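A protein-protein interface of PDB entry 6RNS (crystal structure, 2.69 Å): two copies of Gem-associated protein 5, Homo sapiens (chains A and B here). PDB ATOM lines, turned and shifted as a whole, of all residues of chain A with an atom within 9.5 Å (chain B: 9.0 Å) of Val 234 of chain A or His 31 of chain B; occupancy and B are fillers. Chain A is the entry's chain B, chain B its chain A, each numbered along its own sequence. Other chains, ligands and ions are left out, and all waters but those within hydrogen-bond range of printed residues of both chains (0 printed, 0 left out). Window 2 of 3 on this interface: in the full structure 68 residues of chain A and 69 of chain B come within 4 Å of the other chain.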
ATOM      1  N   TYR A 202     -27.445  -7.713 -24.731  1.00  0.00           N
ATOM      2  CA  TYR A 202     -27.769  -8.098 -23.360  1.00  0.00           C
ATOM      3  C   TYR A 202     -28.902  -7.245 -22.802  1.00  0.00           C
ATOM      4  O   TYR A 202     -29.776  -7.750 -22.088  1.00  0.00           O
ATOM      5  CB  TYR A 202     -26.521  -7.994 -22.480  1.00  0.00           C
ATOM      6  CG  TYR A 202     -25.452  -9.015 -22.819  1.00  0.00           C
ATOM      7  CD1 TYR A 202     -25.596 -10.348 -22.455  1.00  0.00           C
ATOM      8  CD2 TYR A 202     -24.303  -8.647 -23.506  1.00  0.00           C
ATOM      9  CE1 TYR A 202     -24.627 -11.286 -22.767  1.00  0.00           C
ATOM     10  CE2 TYR A 202     -23.328  -9.578 -23.823  1.00  0.00           C
ATOM     11  CZ  TYR A 202     -23.494 -10.896 -23.452  1.00  0.00           C
ATOM     12  OH  TYR A 202     -22.522 -11.820 -23.766  1.00  0.00           O
ATOM     13  N   LEU A 203     -28.917  -5.952 -23.130  1.00  0.00           N
ATOM     14  CA  LEU A 203     -30.040  -5.106 -22.738  1.00  0.00           C
ATOM     15  C   LEU A 203     -31.338  -5.595 -23.378  1.00  0.00           C
ATOM     16  O   LEU A 203     -32.375  -5.692 -22.713  1.00  0.00           O
ATOM     17  CB  LEU A 203     -29.757  -3.654 -23.118  1.00  0.00           C
ATOM     18  CG  LEU A 203     -28.867  -2.870 -22.153  1.00  0.00           C
ATOM     19  CD1 LEU A 203     -28.455  -1.543 -22.769  1.00  0.00           C
ATOM     20  CD2 LEU A 203     -29.582  -2.644 -20.829  1.00  0.00           C
ATOM     21  N   THR A 206     -33.017  -8.213 -21.565  1.00  0.00           N
ATOM     22  CA  THR A 206     -33.387  -7.870 -20.199  1.00  0.00           C
ATOM     23  C   THR A 206     -32.359  -8.378 -19.192  1.00  0.00           C
ATOM     24  O   THR A 206     -32.715  -8.780 -18.077  1.00  0.00           O
ATOM     25  CB  THR A 206     -34.787  -8.400 -19.857  1.00  0.00           C
ATOM     26  OG1 THR A 206     -34.729  -9.815 -19.651  1.00  0.00           O
ATOM     27  CG2 THR A 206     -35.762  -8.102 -20.999  1.00  0.00           C
ATOM     28  N   CYS A 207     -31.088  -8.373 -19.585  1.00  0.00           N
ATOM     29  CA  CYS A 207     -29.969  -8.771 -18.736  1.00  0.00           C
ATOM     30  C   CYS A 207     -29.071  -7.546 -18.560  1.00  0.00           C
ATOM     31  O   CYS A 207     -28.042  -7.410 -19.227  1.00  0.00           O
ATOM     32  CB  CYS A 207     -29.198  -9.964 -19.347  1.00  0.00           C
ATOM     33  SG  CYS A 207     -30.070 -11.549 -19.296  1.00  0.00           S
ATOM     34  N   ALA A 208     -29.462  -6.659 -17.641  1.00  0.00           N
ATOM     35  CA  ALA A 208     -28.771  -5.382 -17.495  1.00  0.00           C
ATOM     36  C   ALA A 208     -27.412  -5.542 -16.824  1.00  0.00           C
ATOM     37  O   ALA A 208     -26.448  -4.862 -17.200  1.00  0.00           O
ATOM     38  CB  ALA A 208     -29.642  -4.410 -16.697  1.00  0.00           C
ATOM     39  N   TYR A 209     -27.316  -6.412 -15.817  1.00  0.00           N
ATOM     40  CA  TYR A 209     -26.028  -6.658 -15.177  1.00  0.00           C
ATOM     41  C   TYR A 209     -24.980  -7.034 -16.217  1.00  0.00           C
ATOM     42  O   TYR A 209     -23.913  -6.415 -16.299  1.00  0.00           O
ATOM     43  CB  TYR A 209     -26.163  -7.762 -14.125  1.00  0.00           C
ATOM     44  CG  TYR A 209     -24.916  -7.983 -13.286  1.00  0.00           C
ATOM     45  CD1 TYR A 209     -24.864  -7.579 -11.956  1.00  0.00           C
ATOM     46  CD2 TYR A 209     -23.791  -8.594 -13.827  1.00  0.00           C
ATOM     47  CE1 TYR A 209     -23.725  -7.781 -11.190  1.00  0.00           C
ATOM     48  CE2 TYR A 209     -22.651  -8.796 -13.072  1.00  0.00           C
ATOM     49  CZ  TYR A 209     -22.623  -8.392 -11.756  1.00  0.00           C
ATOM     50  OH  TYR A 209     -21.485  -8.599 -11.011  1.00  0.00           O
ATOM     51  N   ASP A 210     -25.276  -8.052 -17.030  1.00  0.00           N
ATOM     52  CA  ASP A 210     -24.325  -8.494 -18.043  1.00  0.00           C
ATOM     53  C   ASP A 210     -24.080  -7.420 -19.091  1.00  0.00           C
ATOM     54  O   ASP A 210     -22.995  -7.364 -19.679  1.00  0.00           O
ATOM     55  CB  ASP A 210     -24.833  -9.781 -18.688  1.00  0.00           C
ATOM     56  CG  ASP A 210     -24.921 -10.923 -17.698  1.00  0.00           C
ATOM     57  OD1 ASP A 210     -23.912 -11.185 -17.010  1.00  0.00           O
ATOM     58  OD2 ASP A 210     -26.000 -11.545 -17.592  1.00  0.00           O
ATOM     59  N   ALA A 211     -25.067  -6.555 -19.336  1.00  0.00           N
ATOM     60  CA  ALA A 211     -24.855  -5.431 -20.243  1.00  0.00           C
ATOM     61  C   ALA A 211     -23.774  -4.500 -19.705  1.00  0.00           C
ATOM     62  O   ALA A 211     -22.870  -4.083 -20.440  1.00  0.00           O
ATOM     63  CB  ALA A 211     -26.167  -4.673 -20.452  1.00  0.00           C
ATOM     64  N   ALA A 212     -23.850  -4.166 -18.414  1.00  0.00           N
ATOM     65  CA  ALA A 212     -22.835  -3.312 -17.811  1.00  0.00           C
ATOM     66  C   ALA A 212     -21.470  -3.989 -17.812  1.00  0.00           C
ATOM     67  O   ALA A 212     -20.449  -3.343 -18.074  1.00  0.00           O
ATOM     68  CB  ALA A 212     -23.244  -2.943 -16.384  1.00  0.00           C
ATOM     69  N   THR A 226     -19.699   4.959 -18.973  1.00  0.00           N
ATOM     70  CA  THR A 226     -21.021   4.590 -19.467  1.00  0.00           C
ATOM     71  C   THR A 226     -21.503   3.295 -18.823  1.00  0.00           C
ATOM     72  O   THR A 226     -22.676   3.177 -18.452  1.00  0.00           O
ATOM     73  CB  THR A 226     -20.995   4.450 -20.990  1.00  0.00           C
ATOM     74  OG1 THR A 226     -20.051   3.438 -21.363  1.00  0.00           O
ATOM     75  CG2 THR A 226     -20.612   5.769 -21.649  1.00  0.00           C
ATOM     76  N   ALA A 227     -20.611   2.311 -18.682  1.00  0.00           N
ATOM     77  CA  ALA A 227     -20.975   1.077 -17.995  1.00  0.00           C
ATOM     78  C   ALA A 227     -21.464   1.364 -16.580  1.00  0.00           C
ATOM     79  O   ALA A 227     -22.438   0.759 -16.116  1.00  0.00           O
ATOM     80  CB  ALA A 227     -19.781   0.122 -17.962  1.00  0.00           C
ATOM     81  N   ALA A 228     -20.800   2.288 -15.879  1.00  0.00           N
ATOM     82  CA  ALA A 228     -21.245   2.672 -14.544  1.00  0.00           C
ATOM     83  C   ALA A 228     -22.601   3.366 -14.602  1.00  0.00           C
ATOM     84  O   ALA A 228     -23.517   3.027 -13.843  1.00  0.00           O
ATOM     85  CB  ALA A 228     -20.204   3.578 -13.887  1.00  0.00           C
ATOM     86  N   GLU A 229     -22.749   4.344 -15.501  1.00  0.00           N
ATOM     87  CA  GLU A 229     -24.033   5.018 -15.652  1.00  0.00           C
ATOM     88  C   GLU A 229     -25.130   4.030 -16.029  1.00  0.00           C
ATOM     89  O   GLU A 229     -26.283   4.178 -15.608  1.00  0.00           O
ATOM     90  CB  GLU A 229     -23.922   6.122 -16.703  1.00  0.00           C
ATOM     91  CG  GLU A 229     -22.885   7.185 -16.379  1.00  0.00           C
ATOM     92  CD  GLU A 229     -22.822   8.278 -17.428  1.00  0.00           C
ATOM     93  OE1 GLU A 229     -23.549   8.178 -18.440  1.00  0.00           O
ATOM     94  OE2 GLU A 229     -22.046   9.239 -17.239  1.00  0.00           O
ATOM     95  N   LEU A 230     -24.790   3.012 -16.823  1.00  0.00           N
ATOM     96  CA  LEU A 230     -25.773   2.003 -17.203  1.00  0.00           C
ATOM     97  C   LEU A 230     -26.228   1.200 -15.992  1.00  0.00           C
ATOM     98  O   LEU A 230     -27.423   0.918 -15.840  1.00  0.00           O
ATOM     99  CB  LEU A 230     -25.183   1.083 -18.270  1.00  0.00           C
ATOM    100  CG  LEU A 230     -26.134   0.253 -19.131  1.00  0.00           C
ATOM    101  CD1 LEU A 230     -25.362  -0.290 -20.329  1.00  0.00           C
ATOM    102  CD2 LEU A 230     -26.767  -0.884 -18.360  1.00  0.00           C
ATOM    103  N   ALA A 231     -25.292   0.826 -15.116  1.00  0.00           N
ATOM    104  CA  ALA A 231     -25.652   0.073 -13.920  1.00  0.00           C
ATOM    105  C   ALA A 231     -26.459   0.917 -12.941  1.00  0.00           C
ATOM    106  O   ALA A 231     -27.305   0.383 -12.215  1.00  0.00           O
ATOM    107  CB  ALA A 231     -24.392  -0.466 -13.243  1.00  0.00           C
ATOM    108  N   ALA A 232     -26.213   2.229 -12.901  1.00  0.00           N
ATOM    109  CA  ALA A 232     -26.981   3.097 -12.014  1.00  0.00           C
ATOM    110  C   ALA A 232     -28.426   3.216 -12.487  1.00  0.00           C
ATOM    111  O   ALA A 232     -29.365   3.046 -11.699  1.00  0.00           O
ATOM    112  CB  ALA A 232     -26.324   4.474 -11.929  1.00  0.00           C
ATOM    113  N   ILE A 233     -28.620   3.512 -13.775  1.00  0.00           N
ATOM    114  CA  ILE A 233     -29.965   3.567 -14.347  1.00  0.00           C
ATOM    115  C   ILE A 233     -30.761   2.334 -13.943  1.00  0.00           C
ATOM    116  O   ILE A 233     -31.903   2.427 -13.477  1.00  0.00           O
ATOM    117  CB  ILE A 233     -29.886   3.696 -15.880  1.00  0.00           C
ATOM    118  CG1 ILE A 233     -29.349   5.067 -16.285  1.00  0.00           C
ATOM    119  CG2 ILE A 233     -31.250   3.442 -16.500  1.00  0.00           C
ATOM    120  CD1 ILE A 233     -28.892   5.140 -17.730  1.00  0.00           C
ATOM    121  N   VAL A 234     -30.161   1.155 -14.115  1.00  0.00           N
ATOM    122  CA  VAL A 234     -30.868  -0.095 -13.868  1.00  0.00           C
ATOM    123  C   VAL A 234     -31.163  -0.264 -12.384  1.00  0.00           C
ATOM    124  O   VAL A 234     -32.254  -0.704 -12.002  1.00  0.00           O
ATOM    125  CB  VAL A 234     -30.052  -1.276 -14.425  1.00  0.00           C
ATOM    126  CG1 VAL A 234     -30.450  -2.575 -13.746  1.00  0.00           C
ATOM    127  CG2 VAL A 234     -30.239  -1.366 -15.934  1.00  0.00           C
ATOM    128  N   GLY A 235     -30.205   0.066 -11.527  1.00  0.00           N
ATOM    129  CA  GLY A 235     -30.405  -0.066 -10.099  1.00  0.00           C
ATOM    130  C   GLY A 235     -29.449  -1.039  -9.442  1.00  0.00           C
ATOM    131  O   GLY A 235     -29.653  -1.440  -8.292  1.00  0.00           O
ATOM    132  N   GLU A 236     -28.411  -1.445 -10.168  1.00  0.00           N
ATOM    133  CA  GLU A 236     -27.323  -2.240  -9.596  1.00  0.00           C
ATOM    134  C   GLU A 236     -26.221  -1.303  -9.092  1.00  0.00           C
ATOM    135  O   GLU A 236     -25.072  -1.326  -9.543  1.00  0.00           O
ATOM    136  CB  GLU A 236     -26.784  -3.230 -10.623  1.00  0.00           C
ATOM    137  CG  GLU A 236     -27.835  -4.133 -11.260  1.00  0.00           C
ATOM    138  CD  GLU A 236     -28.339  -5.220 -10.328  1.00  0.00           C
ATOM    139  OE1 GLU A 236     -28.063  -5.141  -9.113  1.00  0.00           O
ATOM    140  OE2 GLU A 236     -29.009  -6.155 -10.813  1.00  0.00           O
ATOM    141  N   ASP A 237     -26.608  -0.453  -8.134  1.00  0.00           N
ATOM    142  CA  ASP A 237     -25.737   0.630  -7.687  1.00  0.00           C
ATOM    143  C   ASP A 237     -24.423   0.119  -7.114  1.00  0.00           C
ATOM    144  O   ASP A 237     -23.390   0.787  -7.249  1.00  0.00           O
ATOM    145  CB  ASP A 237     -26.470   1.480  -6.647  1.00  0.00           C
ATOM    146  CG  ASP A 237     -27.437   2.462  -7.274  1.00  0.00           C
ATOM    147  OD1 ASP A 237     -26.973   3.396  -7.961  1.00  0.00           O
ATOM    148  OD2 ASP A 237     -28.661   2.292  -7.092  1.00  0.00           O
ATOM    149  N   GLU A 238     -24.434  -1.046  -6.468  1.00  0.00           N
ATOM    150  CA  GLU A 238     -23.187  -1.624  -5.978  1.00  0.00           C
ATOM    151  C   GLU A 238     -22.189  -1.792  -7.118  1.00  0.00           C
ATOM    152  O   GLU A 238     -21.025  -1.386  -7.007  1.00  0.00           O
ATOM    153  CB  GLU A 238     -23.464  -2.963  -5.296  1.00  0.00           C
ATOM    154  CG  GLU A 238     -22.247  -3.584  -4.633  1.00  0.00           C
ATOM    155  CD  GLU A 238     -22.607  -4.758  -3.743  1.00  0.00           C
ATOM    156  OE1 GLU A 238     -23.132  -5.765  -4.262  1.00  0.00           O
ATOM    157  OE2 GLU A 238     -22.373  -4.667  -2.519  1.00  0.00           O
ATOM    158  N   LEU A 239     -22.633  -2.380  -8.233  1.00  0.00           N
ATOM    159  CA  LEU A 239     -21.756  -2.548  -9.387  1.00  0.00           C
ATOM    160  C   LEU A 239     -21.414  -1.207 -10.025  1.00  0.00           C
ATOM    161  O   LEU A 239     -20.290  -1.010 -10.500  1.00  0.00           O
ATOM    162  CB  LEU A 239     -22.414  -3.472 -10.413  1.00  0.00           C
ATOM    163  CG  LEU A 239     -21.656  -3.682 -11.724  1.00  0.00           C
ATOM    164  CD1 LEU A 239     -20.333  -4.389 -11.471  1.00  0.00           C
ATOM    165  CD2 LEU A 239     -22.503  -4.469 -12.715  1.00  0.00           C
ATOM    166  N   SER A 240     -22.374  -0.279 -10.059  1.00  0.00           N
ATOM    167  CA  SER A 240     -22.106   1.035 -10.634  1.00  0.00           C
ATOM    168  C   SER A 240     -20.980   1.737  -9.885  1.00  0.00           C
ATOM    169  O   SER A 240     -20.102   2.352 -10.502  1.00  0.00           O
ATOM    170  CB  SER A 240     -23.376   1.886 -10.618  1.00  0.00           C
ATOM    171  OG  SER A 240     -23.668   2.355  -9.313  1.00  0.00           O
ATOM    172  N   CYS B  23     -26.687   2.799 -25.580  1.00  0.00           N
ATOM    173  CA  CYS B  23     -26.828   1.941 -24.408  1.00  0.00           C
ATOM    174  C   CYS B  23     -27.558   2.658 -23.280  1.00  0.00           C
ATOM    175  O   CYS B  23     -28.426   2.070 -22.620  1.00  0.00           O
ATOM    176  CB  CYS B  23     -25.452   1.481 -23.923  1.00  0.00           C
ATOM    177  SG  CYS B  23     -24.626   0.238 -24.943  1.00  0.00           S
ATOM    178  N   LEU B  24     -27.208   3.919 -23.026  1.00  0.00           N
ATOM    179  CA  LEU B  24     -27.884   4.674 -21.979  1.00  0.00           C
ATOM    180  C   LEU B  24     -29.363   4.834 -22.306  1.00  0.00           C
ATOM    181  O   LEU B  24     -30.231   4.548 -21.471  1.00  0.00           O
ATOM    182  CB  LEU B  24     -27.207   6.032 -21.805  1.00  0.00           C
ATOM    183  CG  LEU B  24     -25.717   5.972 -21.454  1.00  0.00           C
ATOM    184  CD1 LEU B  24     -25.105   7.364 -21.443  1.00  0.00           C
ATOM    185  CD2 LEU B  24     -25.504   5.275 -20.116  1.00  0.00           C
ATOM    186  N   VAL B  25     -29.673   5.272 -23.529  1.00  0.00           N
ATOM    187  CA  VAL B  25     -31.067   5.428 -23.935  1.00  0.00           C
ATOM    188  C   VAL B  25     -31.798   4.094 -23.848  1.00  0.00           C
ATOM    189  O   VAL B  25     -32.976   4.035 -23.478  1.00  0.00           O
ATOM    190  CB  VAL B  25     -31.145   6.021 -25.354  1.00  0.00           C
ATOM    191  CG1 VAL B  25     -32.586   6.030 -25.845  1.00  0.00           C
ATOM    192  CG2 VAL B  25     -30.554   7.422 -25.376  1.00  0.00           C
ATOM    193  N   LEU B  26     -31.111   3.002 -24.188  1.00  0.00           N
ATOM    194  CA  LEU B  26     -31.754   1.692 -24.181  1.00  0.00           C
ATOM    195  C   LEU B  26     -32.028   1.222 -22.758  1.00  0.00           C
ATOM    196  O   LEU B  26     -33.094   0.660 -22.482  1.00  0.00           O
ATOM    197  CB  LEU B  26     -30.880   0.691 -24.932  1.00  0.00           C
ATOM    198  CG  LEU B  26     -31.423  -0.723 -25.135  1.00  0.00           C
ATOM    199  CD1 LEU B  26     -32.817  -0.700 -25.726  1.00  0.00           C
ATOM    200  CD2 LEU B  26     -30.467  -1.508 -26.030  1.00  0.00           C
ATOM    201  N   ALA B  27     -31.087   1.453 -21.837  1.00  0.00           N
ATOM    202  CA  ALA B  27     -31.290   1.045 -20.450  1.00  0.00           C
ATOM    203  C   ALA B  27     -32.473   1.775 -19.825  1.00  0.00           C
ATOM    204  O   ALA B  27     -33.261   1.175 -19.084  1.00  0.00           O
ATOM    205  CB  ALA B  27     -30.018   1.300 -19.640  1.00  0.00           C
ATOM    206  N   THR B  28     -32.608   3.072 -20.104  1.00  0.00           N
ATOM    207  CA  THR B  28     -33.762   3.813 -19.614  1.00  0.00           C
ATOM    208  C   THR B  28     -35.061   3.200 -20.121  1.00  0.00           C
ATOM    209  O   THR B  28     -36.031   3.063 -19.365  1.00  0.00           O
ATOM    210  CB  THR B  28     -33.667   5.278 -20.046  1.00  0.00           C
ATOM    211  OG1 THR B  28     -32.399   5.818 -19.647  1.00  0.00           O
ATOM    212  CG2 THR B  28     -34.793   6.096 -19.422  1.00  0.00           C
ATOM    213  N   ALA B  29     -35.098   2.820 -21.400  1.00  0.00           N
ATOM    214  CA  ALA B  29     -36.330   2.314 -21.994  1.00  0.00           C
ATOM    215  C   ALA B  29     -36.744   0.988 -21.366  1.00  0.00           C
ATOM    216  O   ALA B  29     -37.897   0.822 -20.953  1.00  0.00           O
ATOM    217  CB  ALA B  29     -36.155   2.164 -23.506  1.00  0.00           C
ATOM    218  N   LYS B  30     -35.820   0.024 -21.295  1.00  0.00           N
ATOM    219  CA  LYS B  30     -36.165  -1.280 -20.739  1.00  0.00           C
ATOM    220  C   LYS B  30     -36.683  -1.153 -19.313  1.00  0.00           C
ATOM    221  O   LYS B  30     -37.574  -1.909 -18.908  1.00  0.00           O
ATOM    222  CB  LYS B  30     -34.951  -2.215 -20.780  1.00  0.00           C
ATOM    223  CG  LYS B  30     -34.326  -2.419 -22.163  1.00  0.00           C
ATOM    224  CD  LYS B  30     -35.328  -2.926 -23.202  1.00  0.00           C
ATOM    225  CE  LYS B  30     -35.842  -4.327 -22.891  1.00  0.00           C
ATOM    226  NZ  LYS B  30     -36.909  -4.752 -23.852  1.00  0.00           N
ATOM    227  N   HIS B  31     -36.146  -0.200 -18.553  1.00  0.00           N
ATOM    228  CA  HIS B  31     -36.567   0.060 -17.179  1.00  0.00           C
ATOM    229  C   HIS B  31     -37.868   0.863 -17.206  1.00  0.00           C
ATOM    230  O   HIS B  31     -37.915   2.063 -16.925  1.00  0.00           O
ATOM    231  CB  HIS B  31     -35.461   0.795 -16.434  1.00  0.00           C
ATOM    232  CG  HIS B  31     -35.366   0.444 -14.984  1.00  0.00           C
ATOM    233  ND1 HIS B  31     -35.740   1.314 -13.983  1.00  0.00           N
ATOM    234  CD2 HIS B  31     -34.928  -0.678 -14.365  1.00  0.00           C
ATOM    235  CE1 HIS B  31     -35.543   0.740 -12.810  1.00  0.00           C
ATOM    236  NE2 HIS B  31     -35.052  -0.469 -13.013  1.00  0.00           N
ATOM    237  N   SER B  32     -38.950   0.169 -17.558  1.00  0.00           N
ATOM    238  CA  SER B  32     -40.237   0.817 -17.763  1.00  0.00           C
ATOM    239  C   SER B  32     -41.359  -0.012 -17.165  1.00  0.00           C
ATOM    240  O   SER B  32     -41.505  -1.195 -17.488  1.00  0.00           O
ATOM    241  CB  SER B  32     -40.515   1.028 -19.258  1.00  0.00           C
ATOM    242  OG  SER B  32     -40.821  -0.212 -19.880  1.00  0.00           O
ATOM    243  N   ARG B  33     -42.158   0.623 -16.305  1.00  0.00           N
ATOM    244  CA  ARG B  33     -43.397   0.044 -15.812  1.00  0.00           C
ATOM    245  C   ARG B  33     -44.630   0.805 -16.272  1.00  0.00           C
ATOM    246  O   ARG B  33     -45.738   0.265 -16.192  1.00  0.00           O
ATOM    247  CB  ARG B  33     -43.388  -0.015 -14.278  1.00  0.00           C
ATOM    248  CG  ARG B  33     -42.303  -0.914 -13.723  1.00  0.00           C
ATOM    249  CD  ARG B  33     -42.423  -2.308 -14.314  1.00  0.00           C
ATOM    250  NE  ARG B  33     -41.267  -3.142 -14.002  1.00  0.00           N
ATOM    251  CZ  ARG B  33     -41.166  -4.426 -14.327  1.00  0.00           C
ATOM    252  NH1 ARG B  33     -42.157  -5.029 -14.969  1.00  0.00           N
ATOM    253  NH2 ARG B  33     -40.078  -5.111 -14.000  1.00  0.00           N
ATOM    254  N   GLU B  34     -44.459   2.030 -16.753  1.00  0.00           N
ATOM    255  CA  GLU B  34     -45.555   2.865 -17.217  1.00  0.00           C
ATOM    256  C   GLU B  34     -46.395   2.149 -18.270  1.00  0.00           C
ATOM    257  O   GLU B  34     -47.467   2.620 -18.651  1.00  0.00           O
ATOM    258  CB  GLU B  34     -45.003   4.175 -17.779  1.00  0.00           C
ATOM    259  CG  GLU B  34     -43.891   4.780 -16.931  1.00  0.00           C
ATOM    260  CD  GLU B  34     -43.310   6.040 -17.539  1.00  0.00           C
ATOM    261  OE1 GLU B  34     -42.077   6.099 -17.738  1.00  0.00           O
ATOM    262  OE2 GLU B  34     -44.089   6.970 -17.828  1.00  0.00           O
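NE2 of His 31 of chain B sits at hydrogen-bond distance from O of Val 234 of chain A (3.0 Å).
Of the 12 printed residues of chain B, 7 touch a printed residue of chain A.
Printed residues of chain B that touch a printed residue of chain A: Cys 23, Leu 24, Leu 26, Ala 27, Thr 28, Lys 30 and His 31.
Hydrophobic or aromatic side chains of chain B within 4 Å of the printed part of chain A: Leu 24, Leu 26, Ala 27 and His 31.
Of the 24 printed residues of chain A, 5 touch a printed residue of chain B.
Hydrophobic or aromatic side chains of chain A within 4 Å of the printed part of chain B: Leu 203 and Ile 233.
Among the printed residues, 8 pairs touch across the chains.
CD1 of Leu 203 of chain A touches O of Cys 23 of chain B (3.6 Å).
Leu 203 of chain A touches Leu 26 of chain B.
CE of Lys 30 of chain B touches O of Leu 203 of chain A, 3.7 Å away.
Thr 226 of chain A touches Leu 24 of chain B (O to CD2, 3.9 Å).
Glu 229 of chain A touches Leu 24 of chain B.
Ile 233 of chain A touches Ala 27 of chain B.
CG2 of Ile 233 of chain A touches N of Thr 28 of chain B, 3.9 Å away.
Ala 208 of chain A touches none of the printed residues of chain B.
Of the printed residues of chain B, Thr 226 of chain A touches Leu 24 (3.9 Å).
Of chain B, only His 31 (3.0 Å) comes within 4 Å of Val 234 of chain A.
Gly 235 of chain A touches none of the printed residues of chain B.
Printed residues of chain A within 4 Å of Leu 24 of chain B: Thr 226 and Glu 229.
Ala 29 of chain B touches none of the printed residues of chain A.
Of the printed residues of chain A, His 31 of chain B touches Val 234.
The nearest residue of chain A that does not touch His 31 of chain B is Ile 233 of chain A (4.03 Å).
The nearest printed residue of chain B that does not touch Leu 203 of chain A is Ala 27 of chain B (4.1 Å).
No position is printed for both chains.
Of the 8 pairs that touch across the chains among the printed residues, none has its exchanged pair printed and touching as well.
The backbone carbonyl oxygen of Leu 24 of chain B sits at hydrogen-bond distance from the side-chain hydroxyl of Thr 28 of chain B (3.1 Å).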
